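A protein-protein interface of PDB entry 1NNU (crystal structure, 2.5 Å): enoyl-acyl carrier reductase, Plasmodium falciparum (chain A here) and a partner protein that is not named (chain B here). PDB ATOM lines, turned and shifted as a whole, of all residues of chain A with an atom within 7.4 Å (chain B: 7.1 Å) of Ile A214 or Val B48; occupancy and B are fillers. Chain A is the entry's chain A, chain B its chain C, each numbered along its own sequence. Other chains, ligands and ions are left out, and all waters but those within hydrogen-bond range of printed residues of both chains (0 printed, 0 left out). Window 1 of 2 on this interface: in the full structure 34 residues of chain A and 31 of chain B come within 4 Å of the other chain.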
ATOM      1  N   TYR A  15     -19.364 -19.721 -14.177  1.00  0.00           N
ATOM      2  CA  TYR A  15     -19.680 -21.143 -14.244  1.00  0.00           C
ATOM      3  C   TYR A  15     -21.148 -21.394 -14.594  1.00  0.00           C
ATOM      4  O   TYR A  15     -21.477 -22.395 -15.230  1.00  0.00           O
ATOM      5  CB  TYR A  15     -19.360 -21.820 -12.910  1.00  0.00           C
ATOM      6  CG  TYR A  15     -17.922 -22.251 -12.749  1.00  0.00           C
ATOM      7  CD1 TYR A  15     -17.332 -23.122 -13.664  1.00  0.00           C
ATOM      8  CD2 TYR A  15     -17.161 -21.825 -11.658  1.00  0.00           C
ATOM      9  CE1 TYR A  15     -16.028 -23.563 -13.498  1.00  0.00           C
ATOM     10  CE2 TYR A  15     -15.850 -22.263 -11.482  1.00  0.00           C
ATOM     11  CZ  TYR A  15     -15.293 -23.132 -12.407  1.00  0.00           C
ATOM     12  OH  TYR A  15     -14.000 -23.571 -12.239  1.00  0.00           O
ATOM     13  N   ILE A  19     -22.475 -23.997 -17.245  1.00  0.00           N
ATOM     14  CA  ILE A  19     -23.435 -25.031 -16.889  1.00  0.00           C
ATOM     15  C   ILE A  19     -24.628 -24.999 -17.847  1.00  0.00           C
ATOM     16  O   ILE A  19     -25.091 -26.043 -18.311  1.00  0.00           O
ATOM     17  CB  ILE A  19     -23.933 -24.857 -15.428  1.00  0.00           C
ATOM     18  CG1 ILE A  19     -22.764 -25.042 -14.456  1.00  0.00           C
ATOM     19  CG2 ILE A  19     -25.042 -25.848 -15.133  1.00  0.00           C
ATOM     20  CD1 ILE A  19     -23.114 -24.814 -12.993  1.00  0.00           C
ATOM     21  N   ILE A 167     -27.708 -28.864  -7.559  1.00  0.00           N
ATOM     22  CA  ILE A 167     -26.273 -28.729  -7.321  1.00  0.00           C
ATOM     23  C   ILE A 167     -25.942 -27.292  -6.963  1.00  0.00           C
ATOM     24  O   ILE A 167     -26.731 -26.379  -7.200  1.00  0.00           O
ATOM     25  CB  ILE A 167     -25.406 -29.075  -8.543  1.00  0.00           C
ATOM     26  CG1 ILE A 167     -25.773 -28.149  -9.706  1.00  0.00           C
ATOM     27  CG2 ILE A 167     -25.531 -30.551  -8.878  1.00  0.00           C
ATOM     28  CD1 ILE A 167     -24.702 -28.040 -10.771  1.00  0.00           C
ATOM     29  N   SER A 168     -24.765 -27.104  -6.384  1.00  0.00           N
ATOM     30  CA  SER A 168     -24.282 -25.786  -6.020  1.00  0.00           C
ATOM     31  C   SER A 168     -22.778 -25.854  -6.243  1.00  0.00           C
ATOM     32  O   SER A 168     -22.234 -26.935  -6.453  1.00  0.00           O
ATOM     33  CB  SER A 168     -24.593 -25.468  -4.555  1.00  0.00           C
ATOM     34  OG  SER A 168     -23.729 -26.175  -3.689  1.00  0.00           O
ATOM     35  N   LEU A 169     -22.111 -24.706  -6.215  1.00  0.00           N
ATOM     36  CA  LEU A 169     -20.671 -24.671  -6.422  1.00  0.00           C
ATOM     37  C   LEU A 169     -19.950 -24.293  -5.130  1.00  0.00           C
ATOM     38  O   LEU A 169     -20.408 -23.442  -4.375  1.00  0.00           O
ATOM     39  CB  LEU A 169     -20.319 -23.668  -7.524  1.00  0.00           C
ATOM     40  CG  LEU A 169     -20.661 -24.001  -8.978  1.00  0.00           C
ATOM     41  CD1 LEU A 169     -19.988 -25.294  -9.371  1.00  0.00           C
ATOM     42  CD2 LEU A 169     -22.147 -24.128  -9.142  1.00  0.00           C
ATOM     43  N   THR A 170     -18.827 -24.936  -4.865  1.00  0.00           N
ATOM     44  CA  THR A 170     -18.086 -24.622  -3.662  1.00  0.00           C
ATOM     45  C   THR A 170     -16.608 -24.544  -4.012  1.00  0.00           C
ATOM     46  O   THR A 170     -16.220 -24.745  -5.162  1.00  0.00           O
ATOM     47  CB  THR A 170     -18.348 -25.671  -2.531  1.00  0.00           C
ATOM     48  OG1 THR A 170     -17.673 -25.265  -1.333  1.00  0.00           O
ATOM     49  CG2 THR A 170     -17.870 -27.058  -2.943  1.00  0.00           C
ATOM     50  N   TYR A 171     -15.787 -24.224  -3.026  1.00  0.00           N
ATOM     51  CA  TYR A 171     -14.361 -24.095  -3.252  1.00  0.00           C
ATOM     52  C   TYR A 171     -13.634 -24.764  -2.102  1.00  0.00           C
ATOM     53  O   TYR A 171     -14.053 -24.660  -0.949  1.00  0.00           O
ATOM     54  CB  TYR A 171     -13.992 -22.607  -3.350  1.00  0.00           C
ATOM     55  CG  TYR A 171     -12.542 -22.338  -3.672  1.00  0.00           C
ATOM     56  CD1 TYR A 171     -11.918 -22.978  -4.738  1.00  0.00           C
ATOM     57  CD2 TYR A 171     -11.790 -21.455  -2.901  1.00  0.00           C
ATOM     58  CE1 TYR A 171     -10.578 -22.756  -5.025  1.00  0.00           C
ATOM     59  CE2 TYR A 171     -10.446 -21.221  -3.183  1.00  0.00           C
ATOM     60  CZ  TYR A 171      -9.847 -21.880  -4.243  1.00  0.00           C
ATOM     61  OH  TYR A 171      -8.507 -21.696  -4.506  1.00  0.00           O
ATOM     62  N   HIS A 172     -12.551 -25.462  -2.438  1.00  0.00           N
ATOM     63  CA  HIS A 172     -11.715 -26.193  -1.478  1.00  0.00           C
ATOM     64  C   HIS A 172     -11.259 -25.338  -0.285  1.00  0.00           C
ATOM     65  O   HIS A 172     -10.813 -25.876   0.719  1.00  0.00           O
ATOM     66  CB  HIS A 172     -10.503 -26.764  -2.231  1.00  0.00           C
ATOM     67  CG  HIS A 172      -9.756 -27.836  -1.496  1.00  0.00           C
ATOM     68  ND1 HIS A 172     -10.381 -28.931  -0.937  1.00  0.00           N
ATOM     69  CD2 HIS A 172      -8.427 -28.034  -1.322  1.00  0.00           C
ATOM     70  CE1 HIS A 172      -9.470 -29.760  -0.458  1.00  0.00           C
ATOM     71  NE2 HIS A 172      -8.276 -29.240  -0.681  1.00  0.00           N
ATOM     72  N   LYS A 189     -18.592 -21.465   2.477  1.00  0.00           N
ATOM     73  CA  LYS A 189     -18.425 -22.653   1.653  1.00  0.00           C
ATOM     74  C   LYS A 189     -18.425 -23.899   2.532  1.00  0.00           C
ATOM     75  O   LYS A 189     -18.900 -24.963   2.126  1.00  0.00           O
ATOM     76  CB  LYS A 189     -17.128 -22.562   0.843  1.00  0.00           C
ATOM     77  CG  LYS A 189     -17.171 -21.492  -0.252  1.00  0.00           C
ATOM     78  CD  LYS A 189     -18.385 -21.699  -1.170  1.00  0.00           C
ATOM     79  CE  LYS A 189     -18.353 -20.759  -2.360  1.00  0.00           C
ATOM     80  NZ  LYS A 189     -19.546 -20.902  -3.237  1.00  0.00           N
ATOM     81  N   LEU A 192     -21.986 -24.494   3.351  1.00  0.00           N
ATOM     82  CA  LEU A 192     -22.658 -24.980   2.153  1.00  0.00           C
ATOM     83  C   LEU A 192     -22.431 -26.483   1.987  1.00  0.00           C
ATOM     84  O   LEU A 192     -23.374 -27.246   1.767  1.00  0.00           O
ATOM     85  CB  LEU A 192     -22.123 -24.246   0.923  1.00  0.00           C
ATOM     86  CG  LEU A 192     -22.816 -24.526  -0.409  1.00  0.00           C
ATOM     87  CD1 LEU A 192     -24.114 -23.758  -0.465  1.00  0.00           C
ATOM     88  CD2 LEU A 192     -21.930 -24.086  -1.545  1.00  0.00           C
ATOM     89  N   GLU A 193     -21.175 -26.903   2.085  1.00  0.00           N
ATOM     90  CA  GLU A 193     -20.830 -28.315   1.948  1.00  0.00           C
ATOM     91  C   GLU A 193     -21.488 -29.192   3.011  1.00  0.00           C
ATOM     92  O   GLU A 193     -21.936 -30.295   2.710  1.00  0.00           O
ATOM     93  CB  GLU A 193     -19.310 -28.497   1.995  1.00  0.00           C
ATOM     94  CG  GLU A 193     -18.628 -28.172   0.687  1.00  0.00           C
ATOM     95  CD  GLU A 193     -17.126 -28.118   0.810  1.00  0.00           C
ATOM     96  OE1 GLU A 193     -16.560 -28.959   1.538  1.00  0.00           O
ATOM     97  OE2 GLU A 193     -16.512 -27.239   0.168  1.00  0.00           O
ATOM     98  N   THR A 196     -25.281 -29.285   2.485  1.00  0.00           N
ATOM     99  CA  THR A 196     -25.580 -30.151   1.354  1.00  0.00           C
ATOM    100  C   THR A 196     -25.822 -31.570   1.870  1.00  0.00           C
ATOM    101  O   THR A 196     -26.747 -32.259   1.429  1.00  0.00           O
ATOM    102  CB  THR A 196     -24.420 -30.125   0.322  1.00  0.00           C
ATOM    103  OG1 THR A 196     -24.358 -28.828  -0.279  1.00  0.00           O
ATOM    104  CG2 THR A 196     -24.629 -31.170  -0.774  1.00  0.00           C
ATOM    105  N   ASN A 212     -26.301 -32.244  -4.525  1.00  0.00           N
ATOM    106  CA  ASN A 212     -24.856 -32.400  -4.448  1.00  0.00           C
ATOM    107  C   ASN A 212     -24.230 -31.045  -4.705  1.00  0.00           C
ATOM    108  O   ASN A 212     -24.905 -30.108  -5.135  1.00  0.00           O
ATOM    109  CB  ASN A 212     -24.360 -33.404  -5.500  1.00  0.00           C
ATOM    110  CG  ASN A 212     -24.874 -34.819  -5.254  1.00  0.00           C
ATOM    111  OD1 ASN A 212     -24.386 -35.522  -4.376  1.00  0.00           O
ATOM    112  ND2 ASN A 212     -25.872 -35.233  -6.025  1.00  0.00           N
ATOM    113  N   THR A 213     -22.941 -30.934  -4.428  1.00  0.00           N
ATOM    114  CA  THR A 213     -22.241 -29.685  -4.650  1.00  0.00           C
ATOM    115  C   THR A 213     -20.925 -29.985  -5.353  1.00  0.00           C
ATOM    116  O   THR A 213     -20.279 -31.003  -5.090  1.00  0.00           O
ATOM    117  CB  THR A 213     -21.984 -28.945  -3.327  1.00  0.00           C
ATOM    118  OG1 THR A 213     -21.382 -27.683  -3.605  1.00  0.00           O
ATOM    119  CG2 THR A 213     -21.067 -29.746  -2.418  1.00  0.00           C
ATOM    120  N   ILE A 214     -20.547 -29.107  -6.271  1.00  0.00           N
ATOM    121  CA  ILE A 214     -19.318 -29.272  -7.030  1.00  0.00           C
ATOM    122  C   ILE A 214     -18.248 -28.330  -6.500  1.00  0.00           C
ATOM    123  O   ILE A 214     -18.492 -27.137  -6.341  1.00  0.00           O
ATOM    124  CB  ILE A 214     -19.558 -28.975  -8.533  1.00  0.00           C
ATOM    125  CG1 ILE A 214     -20.433 -30.077  -9.140  1.00  0.00           C
ATOM    126  CG2 ILE A 214     -18.236 -28.858  -9.266  1.00  0.00           C
ATOM    127  CD1 ILE A 214     -20.937 -29.766 -10.542  1.00  0.00           C
ATOM    128  N   SER A 215     -17.073 -28.877  -6.205  1.00  0.00           N
ATOM    129  CA  SER A 215     -15.961 -28.071  -5.723  1.00  0.00           C
ATOM    130  C   SER A 215     -15.106 -27.788  -6.964  1.00  0.00           C
ATOM    131  O   SER A 215     -14.313 -28.631  -7.391  1.00  0.00           O
ATOM    132  CB  SER A 215     -15.157 -28.844  -4.673  1.00  0.00           C
ATOM    133  OG  SER A 215     -14.176 -28.018  -4.072  1.00  0.00           O
ATOM    134  N   ALA A 216     -15.272 -26.602  -7.540  1.00  0.00           N
ATOM    135  CA  ALA A 216     -14.549 -26.246  -8.751  1.00  0.00           C
ATOM    136  C   ALA A 216     -13.165 -25.660  -8.558  1.00  0.00           C
ATOM    137  O   ALA A 216     -12.814 -25.178  -7.479  1.00  0.00           O
ATOM    138  CB  ALA A 216     -15.386 -25.288  -9.581  1.00  0.00           C
ATOM    139  N   GLY A 217     -12.390 -25.715  -9.637  1.00  0.00           N
ATOM    140  CA  GLY A 217     -11.053 -25.166  -9.647  1.00  0.00           C
ATOM    141  C   GLY A 217     -11.180 -23.696  -9.987  1.00  0.00           C
ATOM    142  O   GLY A 217     -12.296 -23.200 -10.111  1.00  0.00           O
ATOM    143  N   PRO A 218     -10.064 -22.976 -10.179  1.00  0.00           N
ATOM    144  CA  PRO A 218     -10.079 -21.546 -10.500  1.00  0.00           C
ATOM    145  C   PRO A 218     -10.600 -21.221 -11.891  1.00  0.00           C
ATOM    146  O   PRO A 218     -10.314 -21.931 -12.851  1.00  0.00           O
ATOM    147  CB  PRO A 218      -8.611 -21.134 -10.348  1.00  0.00           C
ATOM    148  CG  PRO A 218      -7.932 -22.322  -9.687  1.00  0.00           C
ATOM    149  CD  PRO A 218      -8.690 -23.490 -10.203  1.00  0.00           C
ATOM    150  N   LEU B  21      -8.601 -25.167 -17.258  1.00  0.00           N
ATOM    151  CA  LEU B  21      -9.895 -25.539 -16.702  1.00  0.00           C
ATOM    152  C   LEU B  21     -10.939 -24.611 -17.298  1.00  0.00           C
ATOM    153  O   LEU B  21     -10.867 -23.393 -17.128  1.00  0.00           O
ATOM    154  CB  LEU B  21      -9.891 -25.409 -15.175  1.00  0.00           C
ATOM    155  CG  LEU B  21     -11.211 -25.794 -14.499  1.00  0.00           C
ATOM    156  CD1 LEU B  21     -11.537 -27.238 -14.811  1.00  0.00           C
ATOM    157  CD2 LEU B  21     -11.111 -25.591 -12.998  1.00  0.00           C
ATOM    158  N   LEU B  22     -11.901 -25.192 -18.005  1.00  0.00           N
ATOM    159  CA  LEU B  22     -12.949 -24.415 -18.653  1.00  0.00           C
ATOM    160  C   LEU B  22     -14.250 -24.479 -17.874  1.00  0.00           C
ATOM    161  O   LEU B  22     -14.521 -25.463 -17.189  1.00  0.00           O
ATOM    162  CB  LEU B  22     -13.187 -24.938 -20.076  1.00  0.00           C
ATOM    163  CG  LEU B  22     -11.990 -24.988 -21.024  1.00  0.00           C
ATOM    164  CD1 LEU B  22     -12.430 -25.604 -22.323  1.00  0.00           C
ATOM    165  CD2 LEU B  22     -11.435 -23.601 -21.261  1.00  0.00           C
ATOM    166  N   ASP B  25     -16.117 -27.519 -18.302  1.00  0.00           N
ATOM    167  CA  ASP B  25     -15.657 -28.755 -17.686  1.00  0.00           C
ATOM    168  C   ASP B  25     -16.573 -28.978 -16.494  1.00  0.00           C
ATOM    169  O   ASP B  25     -17.062 -30.081 -16.268  1.00  0.00           O
ATOM    170  CB  ASP B  25     -14.211 -28.654 -17.210  1.00  0.00           C
ATOM    171  CG  ASP B  25     -13.227 -28.626 -18.353  1.00  0.00           C
ATOM    172  OD1 ASP B  25     -13.495 -29.286 -19.381  1.00  0.00           O
ATOM    173  OD2 ASP B  25     -12.183 -27.960 -18.219  1.00  0.00           O
ATOM    174  N   ILE B  26     -16.807 -27.916 -15.736  1.00  0.00           N
ATOM    175  CA  ILE B  26     -17.698 -28.002 -14.593  1.00  0.00           C
ATOM    176  C   ILE B  26     -19.106 -28.221 -15.128  1.00  0.00           C
ATOM    177  O   ILE B  26     -19.911 -28.935 -14.531  1.00  0.00           O
ATOM    178  CB  ILE B  26     -17.653 -26.702 -13.763  1.00  0.00           C
ATOM    179  CG1 ILE B  26     -16.455 -26.743 -12.811  1.00  0.00           C
ATOM    180  CG2 ILE B  26     -18.957 -26.507 -13.008  1.00  0.00           C
ATOM    181  CD1 ILE B  26     -15.138 -26.978 -13.500  1.00  0.00           C
ATOM    182  N   GLY B  27     -19.383 -27.608 -16.274  1.00  0.00           N
ATOM    183  CA  GLY B  27     -20.692 -27.724 -16.890  1.00  0.00           C
ATOM    184  C   GLY B  27     -21.104 -29.144 -17.213  1.00  0.00           C
ATOM    185  O   GLY B  27     -22.236 -29.543 -16.936  1.00  0.00           O
ATOM    186  N   SER B  28     -20.194 -29.914 -17.796  1.00  0.00           N
ATOM    187  CA  SER B  28     -20.507 -31.287 -18.155  1.00  0.00           C
ATOM    188  C   SER B  28     -20.682 -32.144 -16.910  1.00  0.00           C
ATOM    189  O   SER B  28     -21.461 -33.097 -16.915  1.00  0.00           O
ATOM    190  CB  SER B  28     -19.415 -31.870 -19.048  1.00  0.00           C
ATOM    191  OG  SER B  28     -18.198 -31.937 -18.343  1.00  0.00           O
ATOM    192  N   VAL B  29     -19.969 -31.810 -15.841  1.00  0.00           N
ATOM    193  CA  VAL B  29     -20.109 -32.579 -14.614  1.00  0.00           C
ATOM    194  C   VAL B  29     -21.453 -32.227 -13.965  1.00  0.00           C
ATOM    195  O   VAL B  29     -22.170 -33.107 -13.482  1.00  0.00           O
ATOM    196  CB  VAL B  29     -18.950 -32.308 -13.623  1.00  0.00           C
ATOM    197  CG1 VAL B  29     -19.175 -33.102 -12.352  1.00  0.00           C
ATOM    198  CG2 VAL B  29     -17.616 -32.718 -14.241  1.00  0.00           C
ATOM    199  N   ALA B  30     -21.797 -30.943 -13.970  1.00  0.00           N
ATOM    200  CA  ALA B  30     -23.066 -30.499 -13.411  1.00  0.00           C
ATOM    201  C   ALA B  30     -24.179 -31.261 -14.138  1.00  0.00           C
ATOM    202  O   ALA B  30     -25.037 -31.908 -13.522  1.00  0.00           O
ATOM    203  CB  ALA B  30     -23.231 -29.003 -13.631  1.00  0.00           C
ATOM    204  N   SER B  31     -24.132 -31.181 -15.463  1.00  0.00           N
ATOM    205  CA  SER B  31     -25.101 -31.831 -16.326  1.00  0.00           C
ATOM    206  C   SER B  31     -25.308 -33.297 -15.953  1.00  0.00           C
ATOM    207  O   SER B  31     -26.434 -33.787 -15.923  1.00  0.00           O
ATOM    208  CB  SER B  31     -24.636 -31.717 -17.772  1.00  0.00           C
ATOM    209  OG  SER B  31     -25.604 -32.254 -18.645  1.00  0.00           O
ATOM    210  N   LEU B  33     -24.599 -34.748 -12.947  1.00  0.00           N
ATOM    211  CA  LEU B  33     -25.160 -34.852 -11.600  1.00  0.00           C
ATOM    212  C   LEU B  33     -26.630 -34.454 -11.573  1.00  0.00           C
ATOM    213  O   LEU B  33     -27.374 -34.835 -10.675  1.00  0.00           O
ATOM    214  CB  LEU B  33     -24.391 -33.961 -10.619  1.00  0.00           C
ATOM    215  CG  LEU B  33     -22.993 -34.423 -10.203  1.00  0.00           C
ATOM    216  CD1 LEU B  33     -22.337 -33.359  -9.328  1.00  0.00           C
ATOM    217  CD2 LEU B  33     -23.100 -35.750  -9.460  1.00  0.00           C
ATOM    218  N   GLN B  44     -22.969 -35.339  -1.833  1.00  0.00           N
ATOM    219  CA  GLN B  44     -21.547 -35.387  -2.096  1.00  0.00           C
ATOM    220  C   GLN B  44     -20.956 -34.079  -2.558  1.00  0.00           C
ATOM    221  O   GLN B  44     -21.652 -33.184  -3.035  1.00  0.00           O
ATOM    222  CB  GLN B  44     -21.242 -36.456  -3.151  1.00  0.00           C
ATOM    223  CG  GLN B  44     -21.662 -37.843  -2.741  1.00  0.00           C
ATOM    224  CD  GLN B  44     -21.127 -38.216  -1.374  1.00  0.00           C
ATOM    225  OE1 GLN B  44     -19.915 -38.292  -1.170  1.00  0.00           O
ATOM    226  NE2 GLN B  44     -22.031 -38.440  -0.424  1.00  0.00           N
ATOM    227  N   THR B  45     -19.646 -33.982  -2.386  1.00  0.00           N
ATOM    228  CA  THR B  45     -18.880 -32.831  -2.829  1.00  0.00           C
ATOM    229  C   THR B  45     -17.972 -33.463  -3.870  1.00  0.00           C
ATOM    230  O   THR B  45     -17.073 -34.226  -3.524  1.00  0.00           O
ATOM    231  CB  THR B  45     -18.014 -32.244  -1.698  1.00  0.00           C
ATOM    232  OG1 THR B  45     -18.860 -31.730  -0.667  1.00  0.00           O
ATOM    233  CG2 THR B  45     -17.139 -31.130  -2.223  1.00  0.00           C
ATOM    234  N   ILE B  46     -18.236 -33.192  -5.143  1.00  0.00           N
ATOM    235  CA  ILE B  46     -17.415 -33.758  -6.212  1.00  0.00           C
ATOM    236  C   ILE B  46     -16.396 -32.718  -6.642  1.00  0.00           C
ATOM    237  O   ILE B  46     -16.747 -31.570  -6.909  1.00  0.00           O
ATOM    238  CB  ILE B  46     -18.262 -34.160  -7.448  1.00  0.00           C
ATOM    239  CG1 ILE B  46     -19.354 -35.148  -7.034  1.00  0.00           C
ATOM    240  CG2 ILE B  46     -17.367 -34.784  -8.521  1.00  0.00           C
ATOM    241  CD1 ILE B  46     -18.822 -36.420  -6.417  1.00  0.00           C
ATOM    242  N   TYR B  47     -15.135 -33.117  -6.698  1.00  0.00           N
ATOM    243  CA  TYR B  47     -14.086 -32.205  -7.101  1.00  0.00           C
ATOM    244  C   TYR B  47     -13.839 -32.202  -8.605  1.00  0.00           C
ATOM    245  O   TYR B  47     -13.600 -33.243  -9.216  1.00  0.00           O
ATOM    246  CB  TYR B  47     -12.796 -32.545  -6.356  1.00  0.00           C
ATOM    247  CG  TYR B  47     -12.737 -31.948  -4.967  1.00  0.00           C
ATOM    248  CD1 TYR B  47     -12.089 -30.736  -4.739  1.00  0.00           C
ATOM    249  CD2 TYR B  47     -13.322 -32.601  -3.876  1.00  0.00           C
ATOM    250  CE1 TYR B  47     -12.015 -30.197  -3.466  1.00  0.00           C
ATOM    251  CE2 TYR B  47     -13.257 -32.062  -2.598  1.00  0.00           C
ATOM    252  CZ  TYR B  47     -12.602 -30.865  -2.404  1.00  0.00           C
ATOM    253  OH  TYR B  47     -12.531 -30.323  -1.149  1.00  0.00           O
ATOM    254  N   VAL B  48     -13.913 -31.017  -9.193  1.00  0.00           N
ATOM    255  CA  VAL B  48     -13.679 -30.837 -10.616  1.00  0.00           C
ATOM    256  C   VAL B  48     -12.655 -29.716 -10.642  1.00  0.00           C
ATOM    257  O   VAL B  48     -12.990 -28.544 -10.822  1.00  0.00           O
ATOM    258  CB  VAL B  48     -14.969 -30.410 -11.340  1.00  0.00           C
ATOM    259  CG1 VAL B  48     -14.726 -30.360 -12.844  1.00  0.00           C
ATOM    260  CG2 VAL B  48     -16.101 -31.388 -10.996  1.00  0.00           C
ATOM    261  N   ASP B  49     -11.401 -30.105 -10.446  1.00  0.00           N
ATOM    262  CA  ASP B  49     -10.287 -29.172 -10.349  1.00  0.00           C
ATOM    263  C   ASP B  49      -9.012 -29.777 -10.933  1.00  0.00           C
ATOM    264  O   ASP B  49      -7.920 -29.511 -10.434  1.00  0.00           O
ATOM    265  CB  ASP B  49     -10.044 -28.870  -8.871  1.00  0.00           C
ATOM    266  CG  ASP B  49      -9.583 -30.119  -8.092  1.00  0.00           C
ATOM    267  OD1 ASP B  49      -9.779 -31.250  -8.607  1.00  0.00           O
ATOM    268  OD2 ASP B  49      -9.031 -29.975  -6.972  1.00  0.00           O
ATOM    269  N   ASN B  50      -9.150 -30.594 -11.971  1.00  0.00           N
ATOM    270  CA  ASN B  50      -7.995 -31.241 -12.591  1.00  0.00           C
ATOM    271  C   ASN B  50      -7.169 -32.030 -11.563  1.00  0.00           C
ATOM    272  O   ASN B  50      -6.024 -32.401 -11.817  1.00  0.00           O
ATOM    273  CB  ASN B  50      -7.105 -30.207 -13.308  1.00  0.00           C
ATOM    274  CG  ASN B  50      -7.743 -29.661 -14.584  1.00  0.00           C
ATOM    275  OD1 ASN B  50      -8.467 -30.368 -15.284  1.00  0.00           O
ATOM    276  ND2 ASN B  50      -7.456 -28.405 -14.899  1.00  0.00           N
ATOM    277  N   GLY B  51      -7.765 -32.277 -10.401  1.00  0.00           N
ATOM    278  CA  GLY B  51      -7.096 -33.034  -9.361  1.00  0.00           C
ATOM    279  C   GLY B  51      -6.176 -32.263  -8.428  1.00  0.00           C
ATOM    280  O   GLY B  51      -5.553 -32.862  -7.556  1.00  0.00           O
ATOM    281  N   LEU B  52      -6.088 -30.947  -8.585  1.00  0.00           N
ATOM    282  CA  LEU B  52      -5.205 -30.164  -7.731  1.00  0.00           C
ATOM    283  C   LEU B  52      -5.363 -30.522  -6.247  1.00  0.00           C
ATOM    284  O   LEU B  52      -4.376 -30.623  -5.513  1.00  0.00           O
ATOM    285  CB  LEU B  52      -5.485 -28.673  -7.906  1.00  0.00           C
ATOM    286  CG  LEU B  52      -4.336 -27.660  -7.767  1.00  0.00           C
ATOM    287  CD1 LEU B  52      -4.898 -26.362  -7.204  1.00  0.00           C
ATOM    288  CD2 LEU B  52      -3.228 -28.186  -6.869  1.00  0.00           C
ATOM    289  N   ASN B  53      -6.605 -30.725  -5.811  1.00  0.00           N
ATOM    290  CA  ASN B  53      -6.878 -31.019  -4.409  1.00  0.00           C
ATOM    291  C   ASN B  53      -6.132 -32.218  -3.806  1.00  0.00           C
ATOM    292  O   ASN B  53      -5.976 -32.299  -2.585  1.00  0.00           O
ATOM    293  CB  ASN B  53      -8.392 -31.169  -4.196  1.00  0.00           C
ATOM    294  CG  ASN B  53      -8.923 -32.532  -4.622  1.00  0.00           C
ATOM    295  OD1 ASN B  53      -8.869 -33.493  -3.859  1.00  0.00           O
ATOM    296  ND2 ASN B  53      -9.435 -32.619  -5.841  1.00  0.00           N
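The side-chain amide oxygen of Asn A212 lies within hydrogen-bond range of the backbone NH of Gln B44, at 2.9 Å. The backbone carbonyl oxygen (O) of Thr A213 lies within hydrogen-bond range of the backbone NH (N) of Ile B46 (3.0 Å). The backbone NH (N) of Val B48 is in hydrogen-bond range of the backbone carbonyl oxygen (O) of Ser A215. The backbone carbonyl oxygen of Gln B44 lies within hydrogen-bond range of the backbone NH of Thr A213, at 2.9 Å. A ring nitrogen (ND1) of His A172 lies within hydrogen-bond range of the side-chain hydroxyl (OH) of Tyr B47. O of Ile B46 sits at hydrogen-bond distance from N of Ser A215. The backbone carbonyl oxygen of Val B48 sits at hydrogen-bond distance from the backbone NH of Gly A217 (3.1 Å).
OG1 of Thr A213 is in hydrogen-bond range of OG of Ser A168 (2.8 Å). OD2 of Asp B49 lies within hydrogen-bond range of N of Asn B53 (2.8 Å). N of Ser A168 sits at hydrogen-bond distance from O of Asn A212, 3.3 Å away. OG1 of Thr A170 lies within hydrogen-bond range of OE2 of Glu A193, 2.7 Å away. The backbone NH (N) of Ala A216 is in hydrogen-bond range of the backbone carbonyl oxygen (O) of Thr A170, 3.2 Å away. The backbone NH of Thr A170 lies within hydrogen-bond range of the backbone carbonyl oxygen of Ile A214 (2.7 Å).
Among the printed residues, pairs that only touch across the chains: Tyr A15 with Leu B21, Tyr A15 with Ile B26, Ile A19 with Gly B27, Ile A19 with Ala B30, Ile A167 with Ala B30, Ile A167 with Leu B33, Leu A169 with Ile B26, Glu A193 with Thr B45, Thr A213 with Thr B45, Ile A214 with Ala B30, Ile A214 with Leu B33, Ile A214 with Ile B46, Ile A214 with Val B48, Ser A215 with Thr B45, Ser A215 with Tyr B47, Ala A216 with Ile B26, Ala A216 with Val B48, Gly A217 with Leu B21, Gly A217 with Asp B49 and Pro A218 with Leu B21.
Of the printed residues of chain B, Tyr A15 touches Leu B21 (3.6 Å) and Ile B26 (3.3 Å). Printed residues of chain B within 4 Å of Ile A19: Gly B27 and Ala B30. Printed residues of chain B within 4 Å of Glu A193: Thr B45. Ile A214 touches just these residues of chain B: Ala B30, Leu B33, Ile B46 and Val B48. Ser B28 touches none of the printed residues of chain A. Printed residues of chain A within 4 Å of Leu B33: Ile A167 and Ile A214. Of the printed residues of chain A, Val B48 touches Ile A214, Ser A215, Ala A216 and Gly A217. Printed residues of chain A within 4 Å of Asp B49: Gly A217 (3.9 Å). Leu B52 touches none of the printed residues of chain A. The nearest printed residue of chain B that does not touch Ile A214 is Val B29 (4.2 Å). The nearest printed residue of chain B that does not touch Ile A167 is Ser B31 (5.7 Å).
Printed residues of chain A that touch a printed residue of chain B: Tyr A15, Ile A19, Ile A167, Leu A169, His A172, Glu A193, Asn A212, Thr A213, Ile A214, Ser A215, Ala A216, Gly A217 and Pro A218. Hydrophobic or aromatic side chains of chain A within 4 Å of the printed part of chain B: Tyr A15, Ile A19, Ile A167, Leu A169, His A172, Ile A214 and Ala A216. Hydrophobic or aromatic side chains of chain B that line the printed part of chain A: Leu B21, Ile B26, Ala B30, Leu B33, Tyr B47 and Val B48. Among the printed residues, 27 pairs touch across the chains.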
